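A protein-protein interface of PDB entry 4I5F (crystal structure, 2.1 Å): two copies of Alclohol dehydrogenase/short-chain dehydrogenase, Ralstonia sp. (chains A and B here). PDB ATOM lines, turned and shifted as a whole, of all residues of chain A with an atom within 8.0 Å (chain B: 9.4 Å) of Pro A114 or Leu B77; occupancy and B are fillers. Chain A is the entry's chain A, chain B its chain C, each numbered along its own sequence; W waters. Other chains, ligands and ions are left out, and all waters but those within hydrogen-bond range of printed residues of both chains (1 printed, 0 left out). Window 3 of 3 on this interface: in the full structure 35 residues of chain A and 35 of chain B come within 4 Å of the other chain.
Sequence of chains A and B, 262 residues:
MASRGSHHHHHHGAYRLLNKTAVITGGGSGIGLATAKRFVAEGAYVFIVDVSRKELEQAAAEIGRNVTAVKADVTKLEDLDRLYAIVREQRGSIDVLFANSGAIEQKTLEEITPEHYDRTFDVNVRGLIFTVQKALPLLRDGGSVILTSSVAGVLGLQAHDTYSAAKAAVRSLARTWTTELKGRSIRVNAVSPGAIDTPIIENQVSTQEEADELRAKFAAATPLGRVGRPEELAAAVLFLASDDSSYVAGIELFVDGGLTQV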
ATOM      1  N   GLU A 111     -28.113  12.409  13.121  1.00  0.00           N
ATOM      2  CA  GLU A 111     -27.162  12.837  14.168  1.00  0.00           C
ATOM      3  C   GLU A 111     -25.930  13.495  13.500  1.00  0.00           C
ATOM      4  O   GLU A 111     -25.181  14.221  14.149  1.00  0.00           O
ATOM      5  CB  GLU A 111     -26.684  11.683  15.082  1.00  0.00           C
ATOM      6  CG  GLU A 111     -27.678  11.074  16.042  1.00  0.00           C
ATOM      7  CD  GLU A 111     -27.249   9.648  16.493  1.00  0.00           C
ATOM      8  OE1 GLU A 111     -26.420   8.975  15.795  1.00  0.00           O
ATOM      9  OE2 GLU A 111     -27.758   9.163  17.553  1.00  0.00           O
ATOM     10  N   ILE A 112     -25.755  13.275  12.196  1.00  0.00           N
ATOM     11  CA  ILE A 112     -24.600  13.833  11.499  1.00  0.00           C
ATOM     12  C   ILE A 112     -24.363  15.336  11.703  1.00  0.00           C
ATOM     13  O   ILE A 112     -25.243  16.139  11.412  1.00  0.00           O
ATOM     14  CB  ILE A 112     -24.583  13.488   9.986  1.00  0.00           C
ATOM     15  CG1 ILE A 112     -24.353  11.969   9.792  1.00  0.00           C
ATOM     16  CG2 ILE A 112     -23.561  14.390   9.289  1.00  0.00           C
ATOM     17  CD1 ILE A 112     -24.620  11.491   8.388  1.00  0.00           C
ATOM     18  N   THR A 113     -23.158  15.687  12.187  1.00  0.00           N
ATOM     19  CA  THR A 113     -22.695  17.087  12.266  1.00  0.00           C
ATOM     20  C   THR A 113     -21.635  17.355  11.179  1.00  0.00           C
ATOM     21  O   THR A 113     -20.999  16.425  10.690  1.00  0.00           O
ATOM     22  CB  THR A 113     -22.054  17.445  13.646  1.00  0.00           C
ATOM     23  OG1 THR A 113     -20.814  16.737  13.760  1.00  0.00           O
ATOM     24  CG2 THR A 113     -22.969  17.084  14.798  1.00  0.00           C
ATOM     25  N   PRO A 114     -21.446  18.630  10.810  1.00  0.00           N
ATOM     26  CA  PRO A 114     -20.341  18.981   9.923  1.00  0.00           C
ATOM     27  C   PRO A 114     -18.998  18.452  10.445  1.00  0.00           C
ATOM     28  O   PRO A 114     -18.251  17.836   9.682  1.00  0.00           O
ATOM     29  CB  PRO A 114     -20.378  20.499   9.884  1.00  0.00           C
ATOM     30  CG  PRO A 114     -21.796  20.842  10.159  1.00  0.00           C
ATOM     31  CD  PRO A 114     -22.371  19.754  11.023  1.00  0.00           C
ATOM     32  N   GLU A 115     -18.748  18.596  11.737  1.00  0.00           N
ATOM     33  CA  GLU A 115     -17.514  18.089  12.332  1.00  0.00           C
ATOM     34  C   GLU A 115     -17.350  16.599  12.116  1.00  0.00           C
ATOM     35  O   GLU A 115     -16.312  16.170  11.682  1.00  0.00           O
ATOM     36  CB  GLU A 115     -17.413  18.401  13.827  1.00  0.00           C
ATOM     37  CG  GLU A 115     -17.695  19.854  14.153  1.00  0.00           C
ATOM     38  CD  GLU A 115     -19.215  20.211  14.376  1.00  0.00           C
ATOM     39  OE1 GLU A 115     -19.719  20.155  15.544  1.00  0.00           O
ATOM     40  OE2 GLU A 115     -19.895  20.607  13.391  1.00  0.00           O
ATOM     41  N   HIS A 116     -18.366  15.818  12.425  1.00  0.00           N
ATOM     42  CA  HIS A 116     -18.328  14.392  12.177  1.00  0.00           C
ATOM     43  C   HIS A 116     -18.003  14.007  10.746  1.00  0.00           C
ATOM     44  O   HIS A 116     -17.225  13.076  10.481  1.00  0.00           O
ATOM     45  CB  HIS A 116     -19.675  13.796  12.565  1.00  0.00           C
ATOM     46  CG  HIS A 116     -19.828  12.374  12.158  1.00  0.00           C
ATOM     47  ND1 HIS A 116     -19.262  11.359  12.860  1.00  0.00           N
ATOM     48  CD2 HIS A 116     -20.467  11.808  11.092  1.00  0.00           C
ATOM     49  CE1 HIS A 116     -19.548  10.197  12.290  1.00  0.00           C
ATOM     50  NE2 HIS A 116     -20.273  10.455  11.178  1.00  0.00           N
ATOM     51  N   TYR A 117     -18.661  14.667   9.806  1.00  0.00           N
ATOM     52  CA  TYR A 117     -18.440  14.341   8.372  1.00  0.00           C
ATOM     53  C   TYR A 117     -16.994  14.664   7.937  1.00  0.00           C
ATOM     54  O   TYR A 117     -16.334  13.885   7.238  1.00  0.00           O
ATOM     55  CB  TYR A 117     -19.390  15.198   7.538  1.00  0.00           C
ATOM     56  CG  TYR A 117     -19.073  15.270   6.063  1.00  0.00           C
ATOM     57  CD1 TYR A 117     -19.512  14.273   5.230  1.00  0.00           C
ATOM     58  CD2 TYR A 117     -18.381  16.373   5.509  1.00  0.00           C
ATOM     59  CE1 TYR A 117     -19.265  14.304   3.893  1.00  0.00           C
ATOM     60  CE2 TYR A 117     -18.108  16.442   4.148  1.00  0.00           C
ATOM     61  CZ  TYR A 117     -18.566  15.369   3.340  1.00  0.00           C
ATOM     62  OH  TYR A 117     -18.361  15.329   1.986  1.00  0.00           O
ATOM     63  N   ASP A 118     -16.555  15.862   8.283  1.00  0.00           N
ATOM     64  CA  ASP A 118     -15.213  16.359   7.966  1.00  0.00           C
ATOM     65  C   ASP A 118     -14.092  15.477   8.456  1.00  0.00           C
ATOM     66  O   ASP A 118     -13.192  15.238   7.680  1.00  0.00           O
ATOM     67  CB  ASP A 118     -14.991  17.751   8.566  1.00  0.00           C
ATOM     68  CG  ASP A 118     -15.683  18.805   7.761  1.00  0.00           C
ATOM     69  OD1 ASP A 118     -16.293  18.487   6.724  1.00  0.00           O
ATOM     70  OD2 ASP A 118     -15.651  19.960   8.138  1.00  0.00           O
ATOM     71  N   ARG A 119     -14.154  15.079   9.744  1.00  0.00           N
ATOM     72  CA  ARG A 119     -13.255  14.191  10.394  1.00  0.00           C
ATOM     73  C   ARG A 119     -13.303  12.810   9.721  1.00  0.00           C
ATOM     74  O   ARG A 119     -12.251  12.215   9.436  1.00  0.00           O
ATOM     75  CB  ARG A 119     -13.657  14.042  11.852  1.00  0.00           C
ATOM     76  CG  ARG A 119     -12.756  13.116  12.697  1.00  0.00           C
ATOM     77  CD  ARG A 119     -13.045  13.301  14.204  1.00  0.00           C
ATOM     78  NE  ARG A 119     -14.482  13.212  14.579  1.00  0.00           N
ATOM     79  CZ  ARG A 119     -15.196  14.182  15.183  1.00  0.00           C
ATOM     80  NH1 ARG A 119     -14.636  15.362  15.504  1.00  0.00           N
ATOM     81  NH2 ARG A 119     -16.500  13.977  15.476  1.00  0.00           N
ATOM     82  N   THR A 120     -14.493  12.314   9.400  1.00  0.00           N
ATOM     83  CA  THR A 120     -14.537  10.976   8.733  1.00  0.00           C
ATOM     84  C   THR A 120     -13.896  11.065   7.349  1.00  0.00           C
ATOM     85  O   THR A 120     -13.070  10.227   6.978  1.00  0.00           O
ATOM     86  CB  THR A 120     -15.957  10.435   8.604  1.00  0.00           C
ATOM     87  OG1 THR A 120     -16.529  10.300   9.913  1.00  0.00           O
ATOM     88  CG2 THR A 120     -15.998   8.977   7.838  1.00  0.00           C
ATOM     89  N   PHE A 121     -14.302  12.058   6.549  1.00  0.00           N
ATOM     90  CA  PHE A 121     -13.761  12.160   5.163  1.00  0.00           C
ATOM     91  C   PHE A 121     -12.267  12.526   5.043  1.00  0.00           C
ATOM     92  O   PHE A 121     -11.573  12.033   4.109  1.00  0.00           O
ATOM     93  CB  PHE A 121     -14.694  13.010   4.290  1.00  0.00           C
ATOM     94  CG  PHE A 121     -15.833  12.171   3.697  1.00  0.00           C
ATOM     95  CD1 PHE A 121     -16.924  11.782   4.482  1.00  0.00           C
ATOM     96  CD2 PHE A 121     -15.768  11.688   2.383  1.00  0.00           C
ATOM     97  CE1 PHE A 121     -17.935  10.954   3.982  1.00  0.00           C
ATOM     98  CE2 PHE A 121     -16.773  10.826   1.889  1.00  0.00           C
ATOM     99  CZ  PHE A 121     -17.870  10.488   2.683  1.00  0.00           C
ATOM    100  N   THR A 162     -21.282   7.953   7.103  1.00  0.00           N
ATOM    101  CA  THR A 162     -20.102   8.593   6.466  1.00  0.00           C
ATOM    102  C   THR A 162     -18.961   7.596   6.338  1.00  0.00           C
ATOM    103  O   THR A 162     -18.268   7.593   5.310  1.00  0.00           O
ATOM    104  CB  THR A 162     -19.641   9.869   7.259  1.00  0.00           C
ATOM    105  OG1 THR A 162     -19.275   9.518   8.611  1.00  0.00           O
ATOM    106  CG2 THR A 162     -20.758  10.987   7.255  1.00  0.00           C
ATOM    107  N   ALA B  72     -31.214  28.230  -3.478  1.00  0.00           N
ATOM    108  CA  ALA B  72     -30.475  27.651  -2.373  1.00  0.00           C
ATOM    109  C   ALA B  72     -29.172  27.050  -2.865  1.00  0.00           C
ATOM    110  O   ALA B  72     -29.140  26.462  -3.936  1.00  0.00           O
ATOM    111  CB  ALA B  72     -31.284  26.580  -1.649  1.00  0.00           C
ATOM    112  N   ASP B  73     -28.122  27.211  -2.064  1.00  0.00           N
ATOM    113  CA  ASP B  73     -26.841  26.583  -2.262  1.00  0.00           C
ATOM    114  C   ASP B  73     -26.838  25.459  -1.268  1.00  0.00           C
ATOM    115  O   ASP B  73     -26.667  25.667  -0.057  1.00  0.00           O
ATOM    116  CB  ASP B  73     -25.703  27.573  -1.990  1.00  0.00           C
ATOM    117  CG  ASP B  73     -24.314  26.924  -2.092  1.00  0.00           C
ATOM    118  OD1 ASP B  73     -24.202  25.645  -2.266  1.00  0.00           O
ATOM    119  OD2 ASP B  73     -23.340  27.717  -1.969  1.00  0.00           O
ATOM    120  N   VAL B  74     -27.063  24.248  -1.792  1.00  0.00           N
ATOM    121  CA  VAL B  74     -27.309  23.143  -0.938  1.00  0.00           C
ATOM    122  C   VAL B  74     -26.054  22.756  -0.165  1.00  0.00           C
ATOM    123  O   VAL B  74     -26.126  21.972   0.769  1.00  0.00           O
ATOM    124  CB  VAL B  74     -27.963  21.974  -1.739  1.00  0.00           C
ATOM    125  CG1 VAL B  74     -29.394  22.392  -2.159  1.00  0.00           C
ATOM    126  CG2 VAL B  74     -27.065  21.512  -2.901  1.00  0.00           C
ATOM    127  N   THR B  75     -24.908  23.327  -0.500  1.00  0.00           N
ATOM    128  CA  THR B  75     -23.744  23.127   0.335  1.00  0.00           C
ATOM    129  C   THR B  75     -23.672  24.048   1.544  1.00  0.00           C
ATOM    130  O   THR B  75     -22.646  24.056   2.227  1.00  0.00           O
ATOM    131  CB  THR B  75     -22.381  23.346  -0.419  1.00  0.00           C
ATOM    132  OG1 THR B  75     -22.146  24.741  -0.590  1.00  0.00           O
ATOM    133  CG2 THR B  75     -22.319  22.590  -1.790  1.00  0.00           C
ATOM    134  N   LYS B  76     -24.692  24.885   1.752  1.00  0.00           N
ATOM    135  CA  LYS B  76     -24.731  25.778   2.904  1.00  0.00           C
ATOM    136  C   LYS B  76     -25.915  25.398   3.810  1.00  0.00           C
ATOM    137  O   LYS B  76     -27.115  25.380   3.356  1.00  0.00           O
ATOM    138  CB  LYS B  76     -24.910  27.182   2.426  1.00  0.00           C
ATOM    139  CG  LYS B  76     -23.780  27.687   1.550  1.00  0.00           C
ATOM    140  CD  LYS B  76     -23.972  29.197   1.460  1.00  0.00           C
ATOM    141  CE  LYS B  76     -22.738  29.872   0.889  1.00  0.00           C
ATOM    142  NZ  LYS B  76     -22.956  30.001  -0.584  1.00  0.00           N
ATOM    143  N   LEU B  77     -25.613  25.050   5.069  1.00  0.00           N
ATOM    144  CA  LEU B  77     -26.671  24.487   5.932  1.00  0.00           C
ATOM    145  C   LEU B  77     -27.889  25.398   6.045  1.00  0.00           C
ATOM    146  O   LEU B  77     -29.032  24.923   5.895  1.00  0.00           O
ATOM    147  CB  LEU B  77     -26.180  24.111   7.338  1.00  0.00           C
ATOM    148  CG  LEU B  77     -25.083  23.059   7.484  1.00  0.00           C
ATOM    149  CD1 LEU B  77     -24.675  22.910   8.951  1.00  0.00           C
ATOM    150  CD2 LEU B  77     -25.473  21.744   6.854  1.00  0.00           C
ATOM    151  N   GLU B  78     -27.621  26.688   6.298  1.00  0.00           N
ATOM    152  CA  GLU B  78     -28.649  27.712   6.422  1.00  0.00           C
ATOM    153  C   GLU B  78     -29.510  27.884   5.172  1.00  0.00           C
ATOM    154  O   GLU B  78     -30.725  28.110   5.274  1.00  0.00           O
ATOM    155  CB  GLU B  78     -28.016  29.015   6.852  1.00  0.00           C
ATOM    156  CG  GLU B  78     -27.518  28.856   8.269  1.00  0.00           C
ATOM    157  CD  GLU B  78     -26.323  29.719   8.599  1.00  0.00           C
ATOM    158  OE1 GLU B  78     -26.559  30.940   8.761  1.00  0.00           O
ATOM    159  OE2 GLU B  78     -25.165  29.166   8.684  1.00  0.00           O
ATOM    160  N   ASP B  79     -28.903  27.773   4.002  1.00  0.00           N
ATOM    161  CA  ASP B  79     -29.694  27.743   2.801  1.00  0.00           C
ATOM    162  C   ASP B  79     -30.733  26.582   2.781  1.00  0.00           C
ATOM    163  O   ASP B  79     -31.836  26.774   2.294  1.00  0.00           O
ATOM    164  CB  ASP B  79     -28.791  27.647   1.571  1.00  0.00           C
ATOM    165  CG  ASP B  79     -28.334  28.999   1.025  1.00  0.00           C
ATOM    166  OD1 ASP B  79     -28.243  29.962   1.780  1.00  0.00           O
ATOM    167  OD2 ASP B  79     -28.033  29.089  -0.185  1.00  0.00           O
ATOM    168  N   LEU B  80     -30.371  25.402   3.302  1.00  0.00           N
ATOM    169  CA  LEU B  80     -31.295  24.255   3.377  1.00  0.00           C
ATOM    170  C   LEU B  80     -32.438  24.465   4.427  1.00  0.00           C
ATOM    171  O   LEU B  80     -33.639  24.145   4.184  1.00  0.00           O
ATOM    172  CB  LEU B  80     -30.513  22.933   3.627  1.00  0.00           C
ATOM    173  CG  LEU B  80     -29.611  22.425   2.479  1.00  0.00           C
ATOM    174  CD1 LEU B  80     -28.603  21.390   2.975  1.00  0.00           C
ATOM    175  CD2 LEU B  80     -30.459  21.948   1.306  1.00  0.00           C
ATOM    176  N   ASP B  81     -32.055  24.963   5.590  1.00  0.00           N
ATOM    177  CA  ASP B  81     -33.041  25.513   6.545  1.00  0.00           C
ATOM    178  C   ASP B  81     -34.099  26.364   5.830  1.00  0.00           C
ATOM    179  O   ASP B  81     -35.314  26.145   5.994  1.00  0.00           O
ATOM    180  CB  ASP B  81     -32.333  26.290   7.683  1.00  0.00           C
ATOM    181  CG  ASP B  81     -31.554  25.346   8.592  1.00  0.00           C
ATOM    182  OD1 ASP B  81     -31.573  24.108   8.314  1.00  0.00           O
ATOM    183  OD2 ASP B  81     -30.949  25.791   9.598  1.00  0.00           O
ATOM    184  N   ARG B  82     -33.635  27.280   4.989  1.00  0.00           N
ATOM    185  CA  ARG B  82     -34.554  28.300   4.426  1.00  0.00           C
ATOM    186  C   ARG B  82     -35.391  27.584   3.344  1.00  0.00           C
ATOM    187  O   ARG B  82     -36.591  27.824   3.163  1.00  0.00           O
ATOM    188  CB  ARG B  82     -33.783  29.570   3.972  1.00  0.00           C
ATOM    189  CG  ARG B  82     -34.474  30.360   2.880  1.00  0.00           C
ATOM    190  CD  ARG B  82     -33.907  31.749   2.609  1.00  0.00           C
ATOM    191  NE  ARG B  82     -34.383  32.140   1.270  1.00  0.00           N
ATOM    192  CZ  ARG B  82     -33.772  31.822   0.123  1.00  0.00           C
ATOM    193  NH1 ARG B  82     -32.614  31.150   0.143  1.00  0.00           N
ATOM    194  NH2 ARG B  82     -34.304  32.192  -1.044  1.00  0.00           N
ATOM    195  N   LEU B  83     -34.757  26.647   2.669  1.00  0.00           N
ATOM    196  CA  LEU B  83     -35.469  25.851   1.662  1.00  0.00           C
ATOM    197  C   LEU B  83     -36.630  25.125   2.313  1.00  0.00           C
ATOM    198  O   LEU B  83     -37.818  25.210   1.874  1.00  0.00           O
ATOM    199  CB  LEU B  83     -34.540  24.849   0.992  1.00  0.00           C
ATOM    200  CG  LEU B  83     -35.291  23.756   0.191  1.00  0.00           C
ATOM    201  CD1 LEU B  83     -35.997  24.315  -1.048  1.00  0.00           C
ATOM    202  CD2 LEU B  83     -34.355  22.577  -0.122  1.00  0.00           C
ATOM    203  N   TYR B  84     -36.302  24.374   3.354  1.00  0.00           N
ATOM    204  CA  TYR B  84     -37.356  23.576   3.943  1.00  0.00           C
ATOM    205  C   TYR B  84     -38.422  24.391   4.660  1.00  0.00           C
ATOM    206  O   TYR B  84     -39.570  23.996   4.685  1.00  0.00           O
ATOM    207  CB  TYR B  84     -36.796  22.403   4.745  1.00  0.00           C
ATOM    208  CG  TYR B  84     -36.030  21.463   3.854  1.00  0.00           C
ATOM    209  CD1 TYR B  84     -36.697  20.712   2.867  1.00  0.00           C
ATOM    210  CD2 TYR B  84     -34.645  21.301   3.979  1.00  0.00           C
ATOM    211  CE1 TYR B  84     -36.046  19.829   2.042  1.00  0.00           C
ATOM    212  CE2 TYR B  84     -33.970  20.434   3.143  1.00  0.00           C
ATOM    213  CZ  TYR B  84     -34.670  19.681   2.183  1.00  0.00           C
ATOM    214  OH  TYR B  84     -33.990  18.801   1.352  1.00  0.00           O
ATOM    215  N   ALA B  85     -38.069  25.576   5.177  1.00  0.00           N
ATOM    216  CA  ALA B  85     -39.075  26.409   5.760  1.00  0.00           C
ATOM    217  C   ALA B  85     -40.108  26.843   4.688  1.00  0.00           C
ATOM    218  O   ALA B  85     -41.313  26.887   4.976  1.00  0.00           O
ATOM    219  CB  ALA B  85     -38.447  27.612   6.455  1.00  0.00           C
ATOM    220  N   ASP B 122     -17.838  18.620  -1.385  1.00  0.00           N
ATOM    221  CA  ASP B 122     -18.828  19.432  -0.770  1.00  0.00           C
ATOM    222  C   ASP B 122     -20.116  19.355  -1.600  1.00  0.00           C
ATOM    223  O   ASP B 122     -21.200  19.139  -1.052  1.00  0.00           O
ATOM    224  CB  ASP B 122     -18.397  20.921  -0.628  1.00  0.00           C
ATOM    225  CG  ASP B 122     -17.337  21.151   0.454  1.00  0.00           C
ATOM    226  OD1 ASP B 122     -17.161  20.335   1.368  1.00  0.00           O
ATOM    227  OD2 ASP B 122     -16.679  22.210   0.411  1.00  0.00           O
ATOM    228  N   ARG B 126     -21.160  16.146   0.868  1.00  0.00           N
ATOM    229  CA  ARG B 126     -21.570  16.893   2.055  1.00  0.00           C
ATOM    230  C   ARG B 126     -22.969  17.490   1.854  1.00  0.00           C
ATOM    231  O   ARG B 126     -23.852  17.326   2.692  1.00  0.00           O
ATOM    232  CB  ARG B 126     -20.554  18.000   2.385  1.00  0.00           C
ATOM    233  CG  ARG B 126     -21.042  19.082   3.298  1.00  0.00           C
ATOM    234  CD  ARG B 126     -20.021  20.242   3.375  1.00  0.00           C
ATOM    235  NE  ARG B 126     -19.073  19.951   4.464  1.00  0.00           N
ATOM    236  CZ  ARG B 126     -19.176  20.547   5.633  1.00  0.00           C
ATOM    237  NH1 ARG B 126     -20.116  21.468   5.795  1.00  0.00           N
ATOM    238  NH2 ARG B 126     -18.347  20.260   6.617  1.00  0.00           N
ATOM    239  N   GLY B 127     -23.160  18.211   0.757  1.00  0.00           N
ATOM    240  CA  GLY B 127     -24.435  18.871   0.454  1.00  0.00           C
ATOM    241  C   GLY B 127     -25.602  17.889   0.316  1.00  0.00           C
ATOM    242  O   GLY B 127     -26.700  18.188   0.730  1.00  0.00           O
ATOM    243  N   LEU B 128     -25.346  16.721  -0.242  1.00  0.00           N
ATOM    244  CA  LEU B 128     -26.348  15.731  -0.376  1.00  0.00           C
ATOM    245  C   LEU B 128     -26.775  15.200   0.980  1.00  0.00           C
ATOM    246  O   LEU B 128     -27.969  15.084   1.236  1.00  0.00           O
ATOM    247  CB  LEU B 128     -25.765  14.580  -1.157  1.00  0.00           C
ATOM    248  CG  LEU B 128     -26.761  13.454  -1.410  1.00  0.00           C
ATOM    249  CD1 LEU B 128     -27.321  13.704  -2.794  1.00  0.00           C
ATOM    250  CD2 LEU B 128     -26.029  12.135  -1.332  1.00  0.00           C
ATOM    251  N   ILE B 129     -25.784  14.846   1.828  1.00  0.00           N
ATOM    252  CA  ILE B 129     -26.054  14.398   3.189  1.00  0.00           C
ATOM    253  C   ILE B 129     -27.015  15.334   3.911  1.00  0.00           C
ATOM    254  O   ILE B 129     -28.111  14.919   4.361  1.00  0.00           O
ATOM    255  CB  ILE B 129     -24.791  14.208   4.000  1.00  0.00           C
ATOM    256  CG1 ILE B 129     -24.032  12.962   3.465  1.00  0.00           C
ATOM    257  CG2 ILE B 129     -25.161  14.019   5.444  1.00  0.00           C
ATOM    258  CD1 ILE B 129     -22.589  12.900   3.981  1.00  0.00           C
ATOM    259  N   PHE B 130     -26.607  16.594   4.025  1.00  0.00           N
ATOM    260  CA  PHE B 130     -27.444  17.590   4.649  1.00  0.00           C
ATOM    261  C   PHE B 130     -28.816  17.842   4.005  1.00  0.00           C
ATOM    262  O   PHE B 130     -29.831  18.015   4.703  1.00  0.00           O
ATOM    263  CB  PHE B 130     -26.607  18.877   4.945  1.00  0.00           C
ATOM    264  CG  PHE B 130     -25.597  18.636   6.008  1.00  0.00           C
ATOM    265  CD1 PHE B 130     -26.009  18.255   7.297  1.00  0.00           C
ATOM    266  CD2 PHE B 130     -24.234  18.637   5.729  1.00  0.00           C
ATOM    267  CE1 PHE B 130     -25.065  17.962   8.307  1.00  0.00           C
ATOM    268  CE2 PHE B 130     -23.292  18.317   6.714  1.00  0.00           C
ATOM    269  CZ  PHE B 130     -23.699  17.960   7.994  1.00  0.00           C
ATOM    270  N   THR B 131     -28.846  17.882   2.679  1.00  0.00           N
ATOM    271  CA  THR B 131     -30.094  17.985   1.933  1.00  0.00           C
ATOM    272  C   THR B 131     -31.112  16.943   2.383  1.00  0.00           C
ATOM    273  O   THR B 131     -32.286  17.254   2.565  1.00  0.00           O
ATOM    274  CB  THR B 131     -29.864  17.796   0.415  1.00  0.00           C
ATOM    275  OG1 THR B 131     -29.077  18.876  -0.078  1.00  0.00           O
ATOM    276  CG2 THR B 131     -31.250  17.700  -0.362  1.00  0.00           C
ATOM    277  N   VAL B 132     -30.643  15.728   2.556  1.00  0.00           N
ATOM    278  CA  VAL B 132     -31.489  14.630   2.918  1.00  0.00           C
ATOM    279  C   VAL B 132     -31.774  14.652   4.411  1.00  0.00           C
ATOM    280  O   VAL B 132     -32.946  14.441   4.812  1.00  0.00           O
ATOM    281  CB  VAL B 132     -30.900  13.226   2.472  1.00  0.00           C
ATOM    282  CG1 VAL B 132     -31.807  12.111   2.992  1.00  0.00           C
ATOM    283  CG2 VAL B 132     -30.773  13.126   0.945  1.00  0.00           C
ATOM    284  N   GLN B 133     -30.758  14.903   5.256  1.00  0.00           N
ATOM    285  CA  GLN B 133     -31.015  15.087   6.718  1.00  0.00           C
ATOM    286  C   GLN B 133     -32.152  16.092   7.004  1.00  0.00           C
ATOM    287  O   GLN B 133     -33.003  15.900   7.895  1.00  0.00           O
ATOM    288  CB  GLN B 133     -29.785  15.641   7.442  1.00  0.00           C
ATOM    289  CG  GLN B 133     -29.879  15.679   8.946  1.00  0.00           C
ATOM    290  CD  GLN B 133     -28.663  16.362   9.564  1.00  0.00           C
ATOM    291  OE1 GLN B 133     -28.509  17.593   9.522  1.00  0.00           O
ATOM    292  NE2 GLN B 133     -27.780  15.547  10.140  1.00  0.00           N
ATOM    293  N   LYS B 134     -32.097  17.228   6.344  1.00  0.00           N
ATOM    294  CA  LYS B 134     -33.003  18.274   6.689  1.00  0.00           C
ATOM    295  C   LYS B 134     -34.294  18.056   5.976  1.00  0.00           C
ATOM    296  O   LYS B 134     -35.234  18.721   6.272  1.00  0.00           O
ATOM    297  CB  LYS B 134     -32.415  19.637   6.370  1.00  0.00           C
ATOM    298  CG  LYS B 134     -31.459  20.148   7.444  1.00  0.00           C
ATOM    299  CD  LYS B 134     -30.444  21.116   6.849  1.00  0.00           C
ATOM    300  CE  LYS B 134     -29.353  21.526   7.840  1.00  0.00           C
ATOM    301  NZ  LYS B 134     -29.953  22.211   9.008  1.00  0.00           N
HETATM  302  O   HOH W   1     -16.239  17.904   1.639  1.00  0.00           O
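No position is printed for both chains.
The side-chain amide nitrogen of Gln B133 sits at hydrogen-bond distance from the backbone carbonyl oxygen of Ile A112, 2.9 Å away. The backbone NH of Arg B126 lies within hydrogen-bond range of the side-chain hydroxyl of Tyr A117, at 3.1 Å. The side-chain carboxylate of Asp A118 is in salt-bridge range of the guanidinium group of Arg B126 (2.7 Å).
Of the 24 printed residues of chain B, 5 touch a printed residue of chain A. Hydrophobic or aromatic side chains of chain B within 4 Å of the printed part of chain A: Leu B77, Ile B129 and Phe B130. Of the 12 printed residues of chain A, 5 touch a printed residue of chain B. Hydrophobic or aromatic side chains of chain A that line the printed part of chain B: Ile A112, Pro A114 and Tyr A117. Along chain A the printed residues that touch a printed residue of chain B span positions 112 to 118. Among the printed residues, 10 pairs touch across the chains. Among the printed residues, Asp or Glu carboxylates within 4 Å of a Lys or Arg side-chain nitrogen of the other chain: Asp A118 with Arg B126 (2.7 Å).
Ile A112 touches Ile B129. Ile A112 touches Phe B130 (O to CE1, 3.6 Å). C of Thr A113 touches CZ of Phe B130 (3.8 Å). CG of Pro A114 touches CD1 of Leu B77, at 3.7 Å. Pro A114 touches Arg B126. Phe B130 touches Pro A114 (CZ to N, 3.7 Å). Tyr A117 touches Ile B129.
Of chain B, only Phe B130 comes within 4 Å of Thr A113. Of chain B, only Leu B77 (3.7 Å), Arg B126 (3.9 Å) and Phe B130 (3.7 Å) come within 4 Å of Pro A114. No residue of chain B comes within 4 Å of Glu A115. Of the printed residues of chain B, Tyr A117 touches Arg B126 and Ile B129. Leu B77 touches just one residue of chain A: Pro A114 (3.7 Å). Leu B83 touches none of the printed residues of chain A. Printed residues of chain A within 4 Å of Arg B126: Pro A114, Tyr A117 and Asp A118. Printed residues of chain A within 4 Å of Phe B130: Ile A112, Thr A113 and Pro A114. Of the printed residues of chain A, Gln B133 touches Ile A112 (2.9 Å). The nearest printed residue of chain B that does not touch Ile A112 is Arg B126 (7.2 Å).
The backbone NH (N) of Glu A115 sits close to the side-chain hydroxyl (OG1) of Thr A113 (3.4 Å). OG1 of Thr A113 is in hydrogen-bond range of N of His A116 (2.9 Å). OD1 of Asp B122 is in salt-bridge range of NE of Arg B126 (3.7 Å).
Water W1 bridges OD1 of Asp B122 (2.6 Å) and OH of Tyr A117 (3.4 Å).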
